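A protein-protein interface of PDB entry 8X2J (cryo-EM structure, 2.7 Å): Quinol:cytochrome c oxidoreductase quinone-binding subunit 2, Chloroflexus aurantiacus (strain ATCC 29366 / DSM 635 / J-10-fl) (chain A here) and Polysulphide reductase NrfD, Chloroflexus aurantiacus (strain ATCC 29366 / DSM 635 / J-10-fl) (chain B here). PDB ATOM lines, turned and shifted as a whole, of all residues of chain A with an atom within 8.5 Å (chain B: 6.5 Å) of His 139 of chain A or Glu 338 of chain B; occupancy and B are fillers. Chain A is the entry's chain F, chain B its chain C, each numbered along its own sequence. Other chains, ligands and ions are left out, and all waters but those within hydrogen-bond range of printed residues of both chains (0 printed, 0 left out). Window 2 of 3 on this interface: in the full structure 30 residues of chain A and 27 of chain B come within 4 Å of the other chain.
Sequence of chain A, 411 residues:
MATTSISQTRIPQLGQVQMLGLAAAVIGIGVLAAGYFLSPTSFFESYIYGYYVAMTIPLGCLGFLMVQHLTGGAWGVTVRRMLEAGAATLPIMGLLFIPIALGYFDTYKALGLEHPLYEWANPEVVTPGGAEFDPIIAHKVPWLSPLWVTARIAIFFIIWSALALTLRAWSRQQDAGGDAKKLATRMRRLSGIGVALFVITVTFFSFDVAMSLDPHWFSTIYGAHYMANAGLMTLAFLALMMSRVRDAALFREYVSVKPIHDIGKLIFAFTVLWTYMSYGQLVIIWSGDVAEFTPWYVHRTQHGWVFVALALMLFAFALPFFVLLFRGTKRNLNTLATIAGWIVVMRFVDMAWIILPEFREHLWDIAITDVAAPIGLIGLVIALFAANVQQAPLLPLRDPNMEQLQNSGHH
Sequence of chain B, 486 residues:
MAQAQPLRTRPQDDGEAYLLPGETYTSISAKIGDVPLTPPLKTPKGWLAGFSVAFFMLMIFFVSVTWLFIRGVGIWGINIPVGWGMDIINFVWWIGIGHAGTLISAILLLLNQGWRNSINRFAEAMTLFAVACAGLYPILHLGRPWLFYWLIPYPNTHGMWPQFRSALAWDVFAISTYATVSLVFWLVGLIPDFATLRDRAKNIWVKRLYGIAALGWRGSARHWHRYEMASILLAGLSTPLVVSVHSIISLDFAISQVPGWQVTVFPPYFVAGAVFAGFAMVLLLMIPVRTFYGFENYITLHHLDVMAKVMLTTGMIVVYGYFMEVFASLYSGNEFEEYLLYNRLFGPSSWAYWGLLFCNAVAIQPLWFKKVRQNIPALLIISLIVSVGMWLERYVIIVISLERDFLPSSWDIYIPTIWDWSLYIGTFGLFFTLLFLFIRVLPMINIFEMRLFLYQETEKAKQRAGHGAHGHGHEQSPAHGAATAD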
ATOM      1  N   VAL A 125     -18.167   9.576  28.396  1.00  0.00           N
ATOM      2  CA  VAL A 125     -17.218   8.575  27.921  1.00  0.00           C
ATOM      3  C   VAL A 125     -15.792   9.114  27.932  1.00  0.00           C
ATOM      4  O   VAL A 125     -14.870   8.436  28.393  1.00  0.00           O
ATOM      5  CB  VAL A 125     -17.635   8.077  26.520  1.00  0.00           C
ATOM      6  CG1 VAL A 125     -16.534   7.264  25.861  1.00  0.00           C
ATOM      7  CG2 VAL A 125     -18.903   7.249  26.613  1.00  0.00           C
ATOM      8  N   VAL A 126     -15.573  10.345  27.462  1.00  0.00           N
ATOM      9  CA  VAL A 126     -14.210  10.849  27.313  1.00  0.00           C
ATOM     10  C   VAL A 126     -13.720  11.625  28.529  1.00  0.00           C
ATOM     11  O   VAL A 126     -12.569  12.083  28.528  1.00  0.00           O
ATOM     12  CB  VAL A 126     -14.064  11.706  26.042  1.00  0.00           C
ATOM     13  CG1 VAL A 126     -14.609  10.961  24.852  1.00  0.00           C
ATOM     14  CG2 VAL A 126     -14.738  13.061  26.207  1.00  0.00           C
ATOM     15  N   THR A 127     -14.543  11.783  29.570  1.00  0.00           N
ATOM     16  CA  THR A 127     -13.978  12.440  30.739  1.00  0.00           C
ATOM     17  C   THR A 127     -13.893  11.463  31.904  1.00  0.00           C
ATOM     18  O   THR A 127     -14.779  10.616  32.063  1.00  0.00           O
ATOM     19  CB  THR A 127     -14.805  13.659  31.167  1.00  0.00           C
ATOM     20  OG1 THR A 127     -16.139  13.251  31.487  1.00  0.00           O
ATOM     21  CG2 THR A 127     -14.843  14.699  30.059  1.00  0.00           C
ATOM     22  N   PHE A 133     -16.990   6.292  30.962  1.00  0.00           N
ATOM     23  CA  PHE A 133     -15.532   6.452  31.011  1.00  0.00           C
ATOM     24  C   PHE A 133     -14.818   5.266  30.355  1.00  0.00           C
ATOM     25  O   PHE A 133     -14.175   4.442  31.004  1.00  0.00           O
ATOM     26  CB  PHE A 133     -15.036   6.694  32.442  1.00  0.00           C
ATOM     27  CG  PHE A 133     -13.572   7.048  32.526  1.00  0.00           C
ATOM     28  CD1 PHE A 133     -12.964   7.810  31.537  1.00  0.00           C
ATOM     29  CD2 PHE A 133     -12.804   6.606  33.592  1.00  0.00           C
ATOM     30  CE1 PHE A 133     -11.619   8.119  31.607  1.00  0.00           C
ATOM     31  CE2 PHE A 133     -11.458   6.918  33.674  1.00  0.00           C
ATOM     32  CZ  PHE A 133     -10.867   7.677  32.679  1.00  0.00           C
ATOM     33  N   ASP A 134     -14.993   5.180  29.049  1.00  0.00           N
ATOM     34  CA  ASP A 134     -14.213   4.234  28.269  1.00  0.00           C
ATOM     35  C   ASP A 134     -12.781   4.739  28.168  1.00  0.00           C
ATOM     36  O   ASP A 134     -12.558   5.831  27.627  1.00  0.00           O
ATOM     37  CB  ASP A 134     -14.815   4.062  26.887  1.00  0.00           C
ATOM     38  CG  ASP A 134     -14.582   2.685  26.325  1.00  0.00           C
ATOM     39  OD1 ASP A 134     -14.171   1.785  27.084  1.00  0.00           O
ATOM     40  OD2 ASP A 134     -14.820   2.500  25.122  1.00  0.00           O
ATOM     41  N   PRO A 135     -11.791   3.993  28.669  1.00  0.00           N
ATOM     42  CA  PRO A 135     -10.422   4.529  28.706  1.00  0.00           C
ATOM     43  C   PRO A 135      -9.756   4.604  27.345  1.00  0.00           C
ATOM     44  O   PRO A 135      -8.889   5.460  27.152  1.00  0.00           O
ATOM     45  CB  PRO A 135      -9.694   3.556  29.643  1.00  0.00           C
ATOM     46  CG  PRO A 135     -10.464   2.296  29.540  1.00  0.00           C
ATOM     47  CD  PRO A 135     -11.892   2.685  29.335  1.00  0.00           C
ATOM     48  N   ILE A 136     -10.155   3.768  26.387  1.00  0.00           N
ATOM     49  CA  ILE A 136      -9.568   3.821  25.050  1.00  0.00           C
ATOM     50  C   ILE A 136     -10.040   5.074  24.308  1.00  0.00           C
ATOM     51  O   ILE A 136      -9.243   5.816  23.708  1.00  0.00           O
ATOM     52  CB  ILE A 136      -9.916   2.532  24.286  1.00  0.00           C
ATOM     53  CG1 ILE A 136      -9.527   1.308  25.116  1.00  0.00           C
ATOM     54  CG2 ILE A 136      -9.177   2.463  22.986  1.00  0.00           C
ATOM     55  CD1 ILE A 136      -8.049   1.221  25.440  1.00  0.00           C
ATOM     56  N   ILE A 137     -11.347   5.342  24.368  1.00  0.00           N
ATOM     57  CA  ILE A 137     -11.908   6.547  23.766  1.00  0.00           C
ATOM     58  C   ILE A 137     -11.415   7.792  24.496  1.00  0.00           C
ATOM     59  O   ILE A 137     -11.168   8.834  23.877  1.00  0.00           O
ATOM     60  CB  ILE A 137     -13.445   6.452  23.752  1.00  0.00           C
ATOM     61  CG1 ILE A 137     -13.886   5.114  23.160  1.00  0.00           C
ATOM     62  CG2 ILE A 137     -14.052   7.597  22.968  1.00  0.00           C
ATOM     63  CD1 ILE A 137     -15.383   4.978  22.992  1.00  0.00           C
ATOM     64  N   ALA A 138     -11.238   7.701  25.817  1.00  0.00           N
ATOM     65  CA  ALA A 138     -10.661   8.817  26.559  1.00  0.00           C
ATOM     66  C   ALA A 138      -9.178   8.994  26.251  1.00  0.00           C
ATOM     67  O   ALA A 138      -8.637  10.091  26.426  1.00  0.00           O
ATOM     68  CB  ALA A 138     -10.872   8.618  28.057  1.00  0.00           C
ATOM     69  N   HIS A 139      -8.505   7.926  25.819  1.00  0.00           N
ATOM     70  CA  HIS A 139      -7.131   8.046  25.353  1.00  0.00           C
ATOM     71  C   HIS A 139      -7.068   8.805  24.038  1.00  0.00           C
ATOM     72  O   HIS A 139      -6.133   9.581  23.806  1.00  0.00           O
ATOM     73  CB  HIS A 139      -6.504   6.658  25.212  1.00  0.00           C
ATOM     74  CG  HIS A 139      -5.270   6.633  24.368  1.00  0.00           C
ATOM     75  ND1 HIS A 139      -5.291   6.296  23.032  1.00  0.00           N
ATOM     76  CD2 HIS A 139      -3.977   6.901  24.668  1.00  0.00           C
ATOM     77  CE1 HIS A 139      -4.066   6.361  22.546  1.00  0.00           C
ATOM     78  NE2 HIS A 139      -3.250   6.725  23.517  1.00  0.00           N
ATOM     79  N   LYS A 140      -8.065   8.618  23.171  1.00  0.00           N
ATOM     80  CA  LYS A 140      -8.101   9.363  21.914  1.00  0.00           C
ATOM     81  C   LYS A 140      -8.846  10.691  22.017  1.00  0.00           C
ATOM     82  O   LYS A 140      -9.377  11.161  21.005  1.00  0.00           O
ATOM     83  CB  LYS A 140      -8.729   8.514  20.814  1.00  0.00           C
ATOM     84  CG  LYS A 140      -8.216   7.113  20.751  1.00  0.00           C
ATOM     85  CD  LYS A 140      -9.066   6.304  19.820  1.00  0.00           C
ATOM     86  CE  LYS A 140      -9.155   4.894  20.298  1.00  0.00           C
ATOM     87  NZ  LYS A 140      -9.231   3.913  19.193  1.00  0.00           N
ATOM     88  N   VAL A 141      -8.904  11.311  23.195  1.00  0.00           N
ATOM     89  CA  VAL A 141      -9.705  12.525  23.392  1.00  0.00           C
ATOM     90  C   VAL A 141      -9.202  13.762  22.631  1.00  0.00           C
ATOM     91  O   VAL A 141     -10.058  14.560  22.222  1.00  0.00           O
ATOM     92  CB  VAL A 141      -9.907  12.812  24.902  1.00  0.00           C
ATOM     93  CG1 VAL A 141      -8.650  13.283  25.628  1.00  0.00           C
ATOM     94  CG2 VAL A 141     -11.076  13.774  25.155  1.00  0.00           C
ATOM     95  N   PRO A 142      -7.864  14.018  22.351  1.00  0.00           N
ATOM     96  CA  PRO A 142      -7.590  15.181  21.492  1.00  0.00           C
ATOM     97  C   PRO A 142      -7.894  14.903  20.028  1.00  0.00           C
ATOM     98  O   PRO A 142      -8.509  15.732  19.353  1.00  0.00           O
ATOM     99  CB  PRO A 142      -6.096  15.458  21.717  1.00  0.00           C
ATOM    100  CG  PRO A 142      -5.697  14.604  22.860  1.00  0.00           C
ATOM    101  CD  PRO A 142      -6.571  13.419  22.743  1.00  0.00           C
ATOM    102  N   TRP A 143      -7.484  13.728  19.540  1.00  0.00           N
ATOM    103  CA  TRP A 143      -7.642  13.393  18.127  1.00  0.00           C
ATOM    104  C   TRP A 143      -9.105  13.182  17.762  1.00  0.00           C
ATOM    105  O   TRP A 143      -9.590  13.720  16.762  1.00  0.00           O
ATOM    106  CB  TRP A 143      -6.822  12.148  17.797  1.00  0.00           C
ATOM    107  CG  TRP A 143      -6.717  11.866  16.341  1.00  0.00           C
ATOM    108  CD1 TRP A 143      -7.332  10.863  15.658  1.00  0.00           C
ATOM    109  CD2 TRP A 143      -5.949  12.596  15.379  1.00  0.00           C
ATOM    110  NE1 TRP A 143      -6.996  10.919  14.330  1.00  0.00           N
ATOM    111  CE2 TRP A 143      -6.147  11.976  14.132  1.00  0.00           C
ATOM    112  CE3 TRP A 143      -5.114  13.714  15.451  1.00  0.00           C
ATOM    113  CZ2 TRP A 143      -5.541  12.434  12.967  1.00  0.00           C
ATOM    114  CZ3 TRP A 143      -4.514  14.169  14.295  1.00  0.00           C
ATOM    115  CH2 TRP A 143      -4.730  13.529  13.069  1.00  0.00           C
ATOM    116  N   LEU A 144      -9.825  12.399  18.562  1.00  0.00           N
ATOM    117  CA  LEU A 144     -11.250  12.177  18.351  1.00  0.00           C
ATOM    118  C   LEU A 144     -12.013  13.121  19.276  1.00  0.00           C
ATOM    119  O   LEU A 144     -12.546  12.736  20.314  1.00  0.00           O
ATOM    120  CB  LEU A 144     -11.614  10.717  18.590  1.00  0.00           C
ATOM    121  CG  LEU A 144     -11.110   9.705  17.560  1.00  0.00           C
ATOM    122  CD1 LEU A 144     -11.724   8.345  17.825  1.00  0.00           C
ATOM    123  CD2 LEU A 144     -11.414  10.163  16.145  1.00  0.00           C
ATOM    124  N   PRO A 215     -14.566   3.562  18.317  1.00  0.00           N
ATOM    125  CA  PRO A 215     -13.127   3.741  18.531  1.00  0.00           C
ATOM    126  C   PRO A 215     -12.420   2.533  19.128  1.00  0.00           C
ATOM    127  O   PRO A 215     -11.194   2.565  19.256  1.00  0.00           O
ATOM    128  CB  PRO A 215     -13.068   4.941  19.493  1.00  0.00           C
ATOM    129  CG  PRO A 215     -14.417   5.585  19.407  1.00  0.00           C
ATOM    130  CD  PRO A 215     -15.360   4.460  19.168  1.00  0.00           C
ATOM    131  N   SER B 329      -0.328   3.022  15.976  1.00  0.00           N
ATOM    132  CA  SER B 329       0.319   3.005  17.285  1.00  0.00           C
ATOM    133  C   SER B 329      -0.160   4.151  18.172  1.00  0.00           C
ATOM    134  O   SER B 329      -0.377   3.959  19.373  1.00  0.00           O
ATOM    135  CB  SER B 329       1.835   3.058  17.118  1.00  0.00           C
ATOM    136  OG  SER B 329       2.330   1.849  16.570  1.00  0.00           O
ATOM    137  N   LEU B 330      -0.335   5.346  17.604  1.00  0.00           N
ATOM    138  CA  LEU B 330      -0.772   6.485  18.410  1.00  0.00           C
ATOM    139  C   LEU B 330      -2.266   6.432  18.720  1.00  0.00           C
ATOM    140  O   LEU B 330      -2.691   6.840  19.803  1.00  0.00           O
ATOM    141  CB  LEU B 330      -0.428   7.791  17.696  1.00  0.00           C
ATOM    142  CG  LEU B 330       1.041   8.201  17.716  1.00  0.00           C
ATOM    143  CD1 LEU B 330       1.304   9.253  16.659  1.00  0.00           C
ATOM    144  CD2 LEU B 330       1.419   8.714  19.089  1.00  0.00           C
ATOM    145  N   TYR B 331      -3.066   5.936  17.780  1.00  0.00           N
ATOM    146  CA  TYR B 331      -4.514   5.873  17.896  1.00  0.00           C
ATOM    147  C   TYR B 331      -4.957   4.748  18.811  1.00  0.00           C
ATOM    148  O   TYR B 331      -5.969   4.882  19.506  1.00  0.00           O
ATOM    149  CB  TYR B 331      -5.104   5.690  16.496  1.00  0.00           C
ATOM    150  CG  TYR B 331      -6.609   5.707  16.379  1.00  0.00           C
ATOM    151  CD1 TYR B 331      -7.321   6.898  16.466  1.00  0.00           C
ATOM    152  CD2 TYR B 331      -7.314   4.536  16.136  1.00  0.00           C
ATOM    153  CE1 TYR B 331      -8.694   6.915  16.332  1.00  0.00           C
ATOM    154  CE2 TYR B 331      -8.684   4.543  16.008  1.00  0.00           C
ATOM    155  CZ  TYR B 331      -9.370   5.733  16.110  1.00  0.00           C
ATOM    156  OH  TYR B 331     -10.738   5.736  15.980  1.00  0.00           O
ATOM    157  N   SER B 332      -4.220   3.642  18.822  1.00  0.00           N
ATOM    158  CA  SER B 332      -4.541   2.539  19.709  1.00  0.00           C
ATOM    159  C   SER B 332      -4.228   2.908  21.150  1.00  0.00           C
ATOM    160  O   SER B 332      -3.231   3.577  21.436  1.00  0.00           O
ATOM    161  CB  SER B 332      -3.736   1.309  19.315  1.00  0.00           C
ATOM    162  OG  SER B 332      -3.824   1.094  17.926  1.00  0.00           O
ATOM    163  N   GLY B 333      -5.071   2.447  22.065  1.00  0.00           N
ATOM    164  CA  GLY B 333      -4.714   2.466  23.464  1.00  0.00           C
ATOM    165  C   GLY B 333      -3.900   1.274  23.902  1.00  0.00           C
ATOM    166  O   GLY B 333      -3.702   1.062  25.100  1.00  0.00           O
ATOM    167  N   ASN B 334      -3.425   0.483  22.942  1.00  0.00           N
ATOM    168  CA  ASN B 334      -2.751  -0.771  23.222  1.00  0.00           C
ATOM    169  C   ASN B 334      -1.301  -0.501  23.598  1.00  0.00           C
ATOM    170  O   ASN B 334      -0.570   0.168  22.858  1.00  0.00           O
ATOM    171  CB  ASN B 334      -2.831  -1.683  22.000  1.00  0.00           C
ATOM    172  CG  ASN B 334      -2.534  -3.125  22.326  1.00  0.00           C
ATOM    173  OD1 ASN B 334      -2.275  -3.472  23.474  1.00  0.00           O
ATOM    174  ND2 ASN B 334      -2.569  -3.978  21.312  1.00  0.00           N
ATOM    175  N   GLU B 335      -0.889  -1.033  24.754  1.00  0.00           N
ATOM    176  CA  GLU B 335       0.467  -0.817  25.248  1.00  0.00           C
ATOM    177  C   GLU B 335       1.507  -1.480  24.358  1.00  0.00           C
ATOM    178  O   GLU B 335       2.631  -0.989  24.252  1.00  0.00           O
ATOM    179  CB  GLU B 335       0.590  -1.325  26.686  1.00  0.00           C
ATOM    180  CG  GLU B 335       1.863  -0.888  27.407  1.00  0.00           C
ATOM    181  CD  GLU B 335       2.128   0.603  27.278  1.00  0.00           C
ATOM    182  OE1 GLU B 335       1.231   1.407  27.615  1.00  0.00           O
ATOM    183  OE2 GLU B 335       3.234   0.973  26.830  1.00  0.00           O
ATOM    184  N   PHE B 336       1.142  -2.562  23.677  1.00  0.00           N
ATOM    185  CA  PHE B 336       2.091  -3.242  22.808  1.00  0.00           C
ATOM    186  C   PHE B 336       2.312  -2.477  21.510  1.00  0.00           C
ATOM    187  O   PHE B 336       3.436  -2.435  21.003  1.00  0.00           O
ATOM    188  CB  PHE B 336       1.618  -4.671  22.552  1.00  0.00           C
ATOM    189  CG  PHE B 336       1.320  -5.424  23.813  1.00  0.00           C
ATOM    190  CD1 PHE B 336       2.336  -6.036  24.527  1.00  0.00           C
ATOM    191  CD2 PHE B 336       0.029  -5.499  24.302  1.00  0.00           C
ATOM    192  CE1 PHE B 336       2.060  -6.713  25.699  1.00  0.00           C
ATOM    193  CE2 PHE B 336      -0.241  -6.158  25.469  1.00  0.00           C
ATOM    194  CZ  PHE B 336       0.770  -6.780  26.163  1.00  0.00           C
ATOM    195  N   GLU B 337       1.270  -1.828  20.982  1.00  0.00           N
ATOM    196  CA  GLU B 337       1.454  -0.936  19.839  1.00  0.00           C
ATOM    197  C   GLU B 337       2.240   0.311  20.233  1.00  0.00           C
ATOM    198  O   GLU B 337       3.108   0.776  19.476  1.00  0.00           O
ATOM    199  CB  GLU B 337       0.099  -0.545  19.257  1.00  0.00           C
ATOM    200  CG  GLU B 337      -0.753  -1.721  18.825  1.00  0.00           C
ATOM    201  CD  GLU B 337      -0.248  -2.366  17.555  1.00  0.00           C
ATOM    202  OE1 GLU B 337       0.249  -1.634  16.673  1.00  0.00           O
ATOM    203  OE2 GLU B 337      -0.345  -3.606  17.441  1.00  0.00           O
ATOM    204  N   GLU B 338       1.949   0.853  21.423  1.00  0.00           N
ATOM    205  CA  GLU B 338       2.682   2.012  21.924  1.00  0.00           C
ATOM    206  C   GLU B 338       4.156   1.689  22.138  1.00  0.00           C
ATOM    207  O   GLU B 338       5.034   2.484  21.777  1.00  0.00           O
ATOM    208  CB  GLU B 338       2.045   2.504  23.222  1.00  0.00           C
ATOM    209  CG  GLU B 338       0.711   3.200  23.036  1.00  0.00           C
ATOM    210  CD  GLU B 338       0.079   3.609  24.351  1.00  0.00           C
ATOM    211  OE1 GLU B 338       0.800   3.651  25.369  1.00  0.00           O
ATOM    212  OE2 GLU B 338      -1.137   3.888  24.369  1.00  0.00           O
ATOM    213  N   TYR B 339       4.454   0.510  22.687  1.00  0.00           N
ATOM    214  CA  TYR B 339       5.840   0.111  22.858  1.00  0.00           C
ATOM    215  C   TYR B 339       6.496  -0.310  21.555  1.00  0.00           C
ATOM    216  O   TYR B 339       7.714  -0.210  21.452  1.00  0.00           O
ATOM    217  CB  TYR B 339       5.976  -1.019  23.880  1.00  0.00           C
ATOM    218  CG  TYR B 339       7.355  -1.042  24.500  1.00  0.00           C
ATOM    219  CD1 TYR B 339       7.679  -0.191  25.545  1.00  0.00           C
ATOM    220  CD2 TYR B 339       8.342  -1.896  24.019  1.00  0.00           C
ATOM    221  CE1 TYR B 339       8.940  -0.194  26.100  1.00  0.00           C
ATOM    222  CE2 TYR B 339       9.606  -1.896  24.559  1.00  0.00           C
ATOM    223  CZ  TYR B 339       9.898  -1.051  25.605  1.00  0.00           C
ATOM    224  OH  TYR B 339      11.156  -1.059  26.158  1.00  0.00           O
ATOM    225  N   LEU B 340       5.732  -0.765  20.560  1.00  0.00           N
ATOM    226  CA  LEU B 340       6.305  -0.989  19.237  1.00  0.00           C
ATOM    227  C   LEU B 340       6.797   0.319  18.630  1.00  0.00           C
ATOM    228  O   LEU B 340       7.914   0.390  18.098  1.00  0.00           O
ATOM    229  CB  LEU B 340       5.273  -1.647  18.326  1.00  0.00           C
ATOM    230  CG  LEU B 340       5.675  -1.696  16.855  1.00  0.00           C
ATOM    231  CD1 LEU B 340       6.623  -2.857  16.598  1.00  0.00           C
ATOM    232  CD2 LEU B 340       4.453  -1.744  15.961  1.00  0.00           C
ATOM    233  N   LEU B 341       5.983   1.376  18.737  1.00  0.00           N
ATOM    234  CA  LEU B 341       6.416   2.693  18.268  1.00  0.00           C
ATOM    235  C   LEU B 341       7.594   3.221  19.080  1.00  0.00           C
ATOM    236  O   LEU B 341       8.541   3.782  18.511  1.00  0.00           O
ATOM    237  CB  LEU B 341       5.259   3.686  18.316  1.00  0.00           C
ATOM    238  CG  LEU B 341       5.480   4.970  17.513  1.00  0.00           C
ATOM    239  CD1 LEU B 341       5.795   4.646  16.062  1.00  0.00           C
ATOM    240  CD2 LEU B 341       4.276   5.886  17.609  1.00  0.00           C
ATOM    241  N   TYR B 342       7.561   3.038  20.405  1.00  0.00           N
ATOM    242  CA  TYR B 342       8.668   3.482  21.251  1.00  0.00           C
ATOM    243  C   TYR B 342       9.949   2.713  20.952  1.00  0.00           C
ATOM    244  O   TYR B 342      11.037   3.292  20.955  1.00  0.00           O
ATOM    245  CB  TYR B 342       8.305   3.336  22.730  1.00  0.00           C
ATOM    246  CG  TYR B 342       9.459   3.653  23.658  1.00  0.00           C
ATOM    247  CD1 TYR B 342       9.863   4.965  23.867  1.00  0.00           C
ATOM    248  CD2 TYR B 342      10.161   2.640  24.306  1.00  0.00           C
ATOM    249  CE1 TYR B 342      10.919   5.261  24.704  1.00  0.00           C
ATOM    250  CE2 TYR B 342      11.224   2.929  25.136  1.00  0.00           C
ATOM    251  CZ  TYR B 342      11.595   4.240  25.333  1.00  0.00           C
ATOM    252  OH  TYR B 342      12.649   4.532  26.165  1.00  0.00           O
ATOM    253  N   ASN B 343       9.840   1.407  20.712  1.00  0.00           N
ATOM    254  CA  ASN B 343      11.002   0.576  20.433  1.00  0.00           C
ATOM    255  C   ASN B 343      11.611   0.920  19.085  1.00  0.00           C
ATOM    256  O   ASN B 343      12.838   0.954  18.948  1.00  0.00           O
ATOM    257  CB  ASN B 343      10.599  -0.897  20.487  1.00  0.00           C
ATOM    258  CG  ASN B 343      11.785  -1.830  20.488  1.00  0.00           C
ATOM    259  OD1 ASN B 343      12.876  -1.469  20.919  1.00  0.00           O
ATOM    260  ND2 ASN B 343      11.576  -3.046  20.001  1.00  0.00           N
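Among the printed residues, pairs that only touch across the chains: His 139 of chain A with Leu 330 of chain B, His 139 of chain A with Ser 332 of chain B, Leu 144 of chain A with Tyr 331 of chain B, His 139 of chain A with Glu 338 of chain B, His 139 of chain A with Tyr 331 of chain B and His 139 of chain A with Gly 333 of chain B.
NZ of Lys 140 of chain A lies close to O of Tyr 331 of chain B, 3.4 Å away.
Of the 15 printed residues of chain B, 5 touch a printed residue of chain A. Along chain B the printed residues that touch a printed residue of chain A span positions 330 to 338. Hydrophobic or aromatic side chains of chain A within 4 Å of the printed part of chain B: His 139 and Leu 144. Among the printed residues, no Asp or Glu carboxylate lies within 4 Å of a Lys or Arg side-chain nitrogen of the other chain.
His 139 of chain A touches just these residues of chain B: Leu 330, Tyr 331, Ser 332, Gly 333 and Glu 338. Of the printed residues of chain B, Lys 140 of chain A touches Tyr 331. Of the printed residues of chain B, Leu 144 of chain A touches Tyr 331 (3.3 Å). Of the printed residues of chain A, Tyr 331 of chain B touches His 139 (3.9 Å), Lys 140 (3.3 Å) and Leu 144 (3.3 Å). Gly 333 of chain B touches just one residue of chain A: His 139 (3.9 Å). Glu 338 of chain B touches just one residue of chain A: His 139 (3.6 Å). The nearest residue of chain A that does not touch Glu 338 of chain B is Ile 136 of chain A (7.5 Å). The nearest printed residue of chain A that does not touch Leu 330 of chain B is Lys 140 of chain A (5.6 Å).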
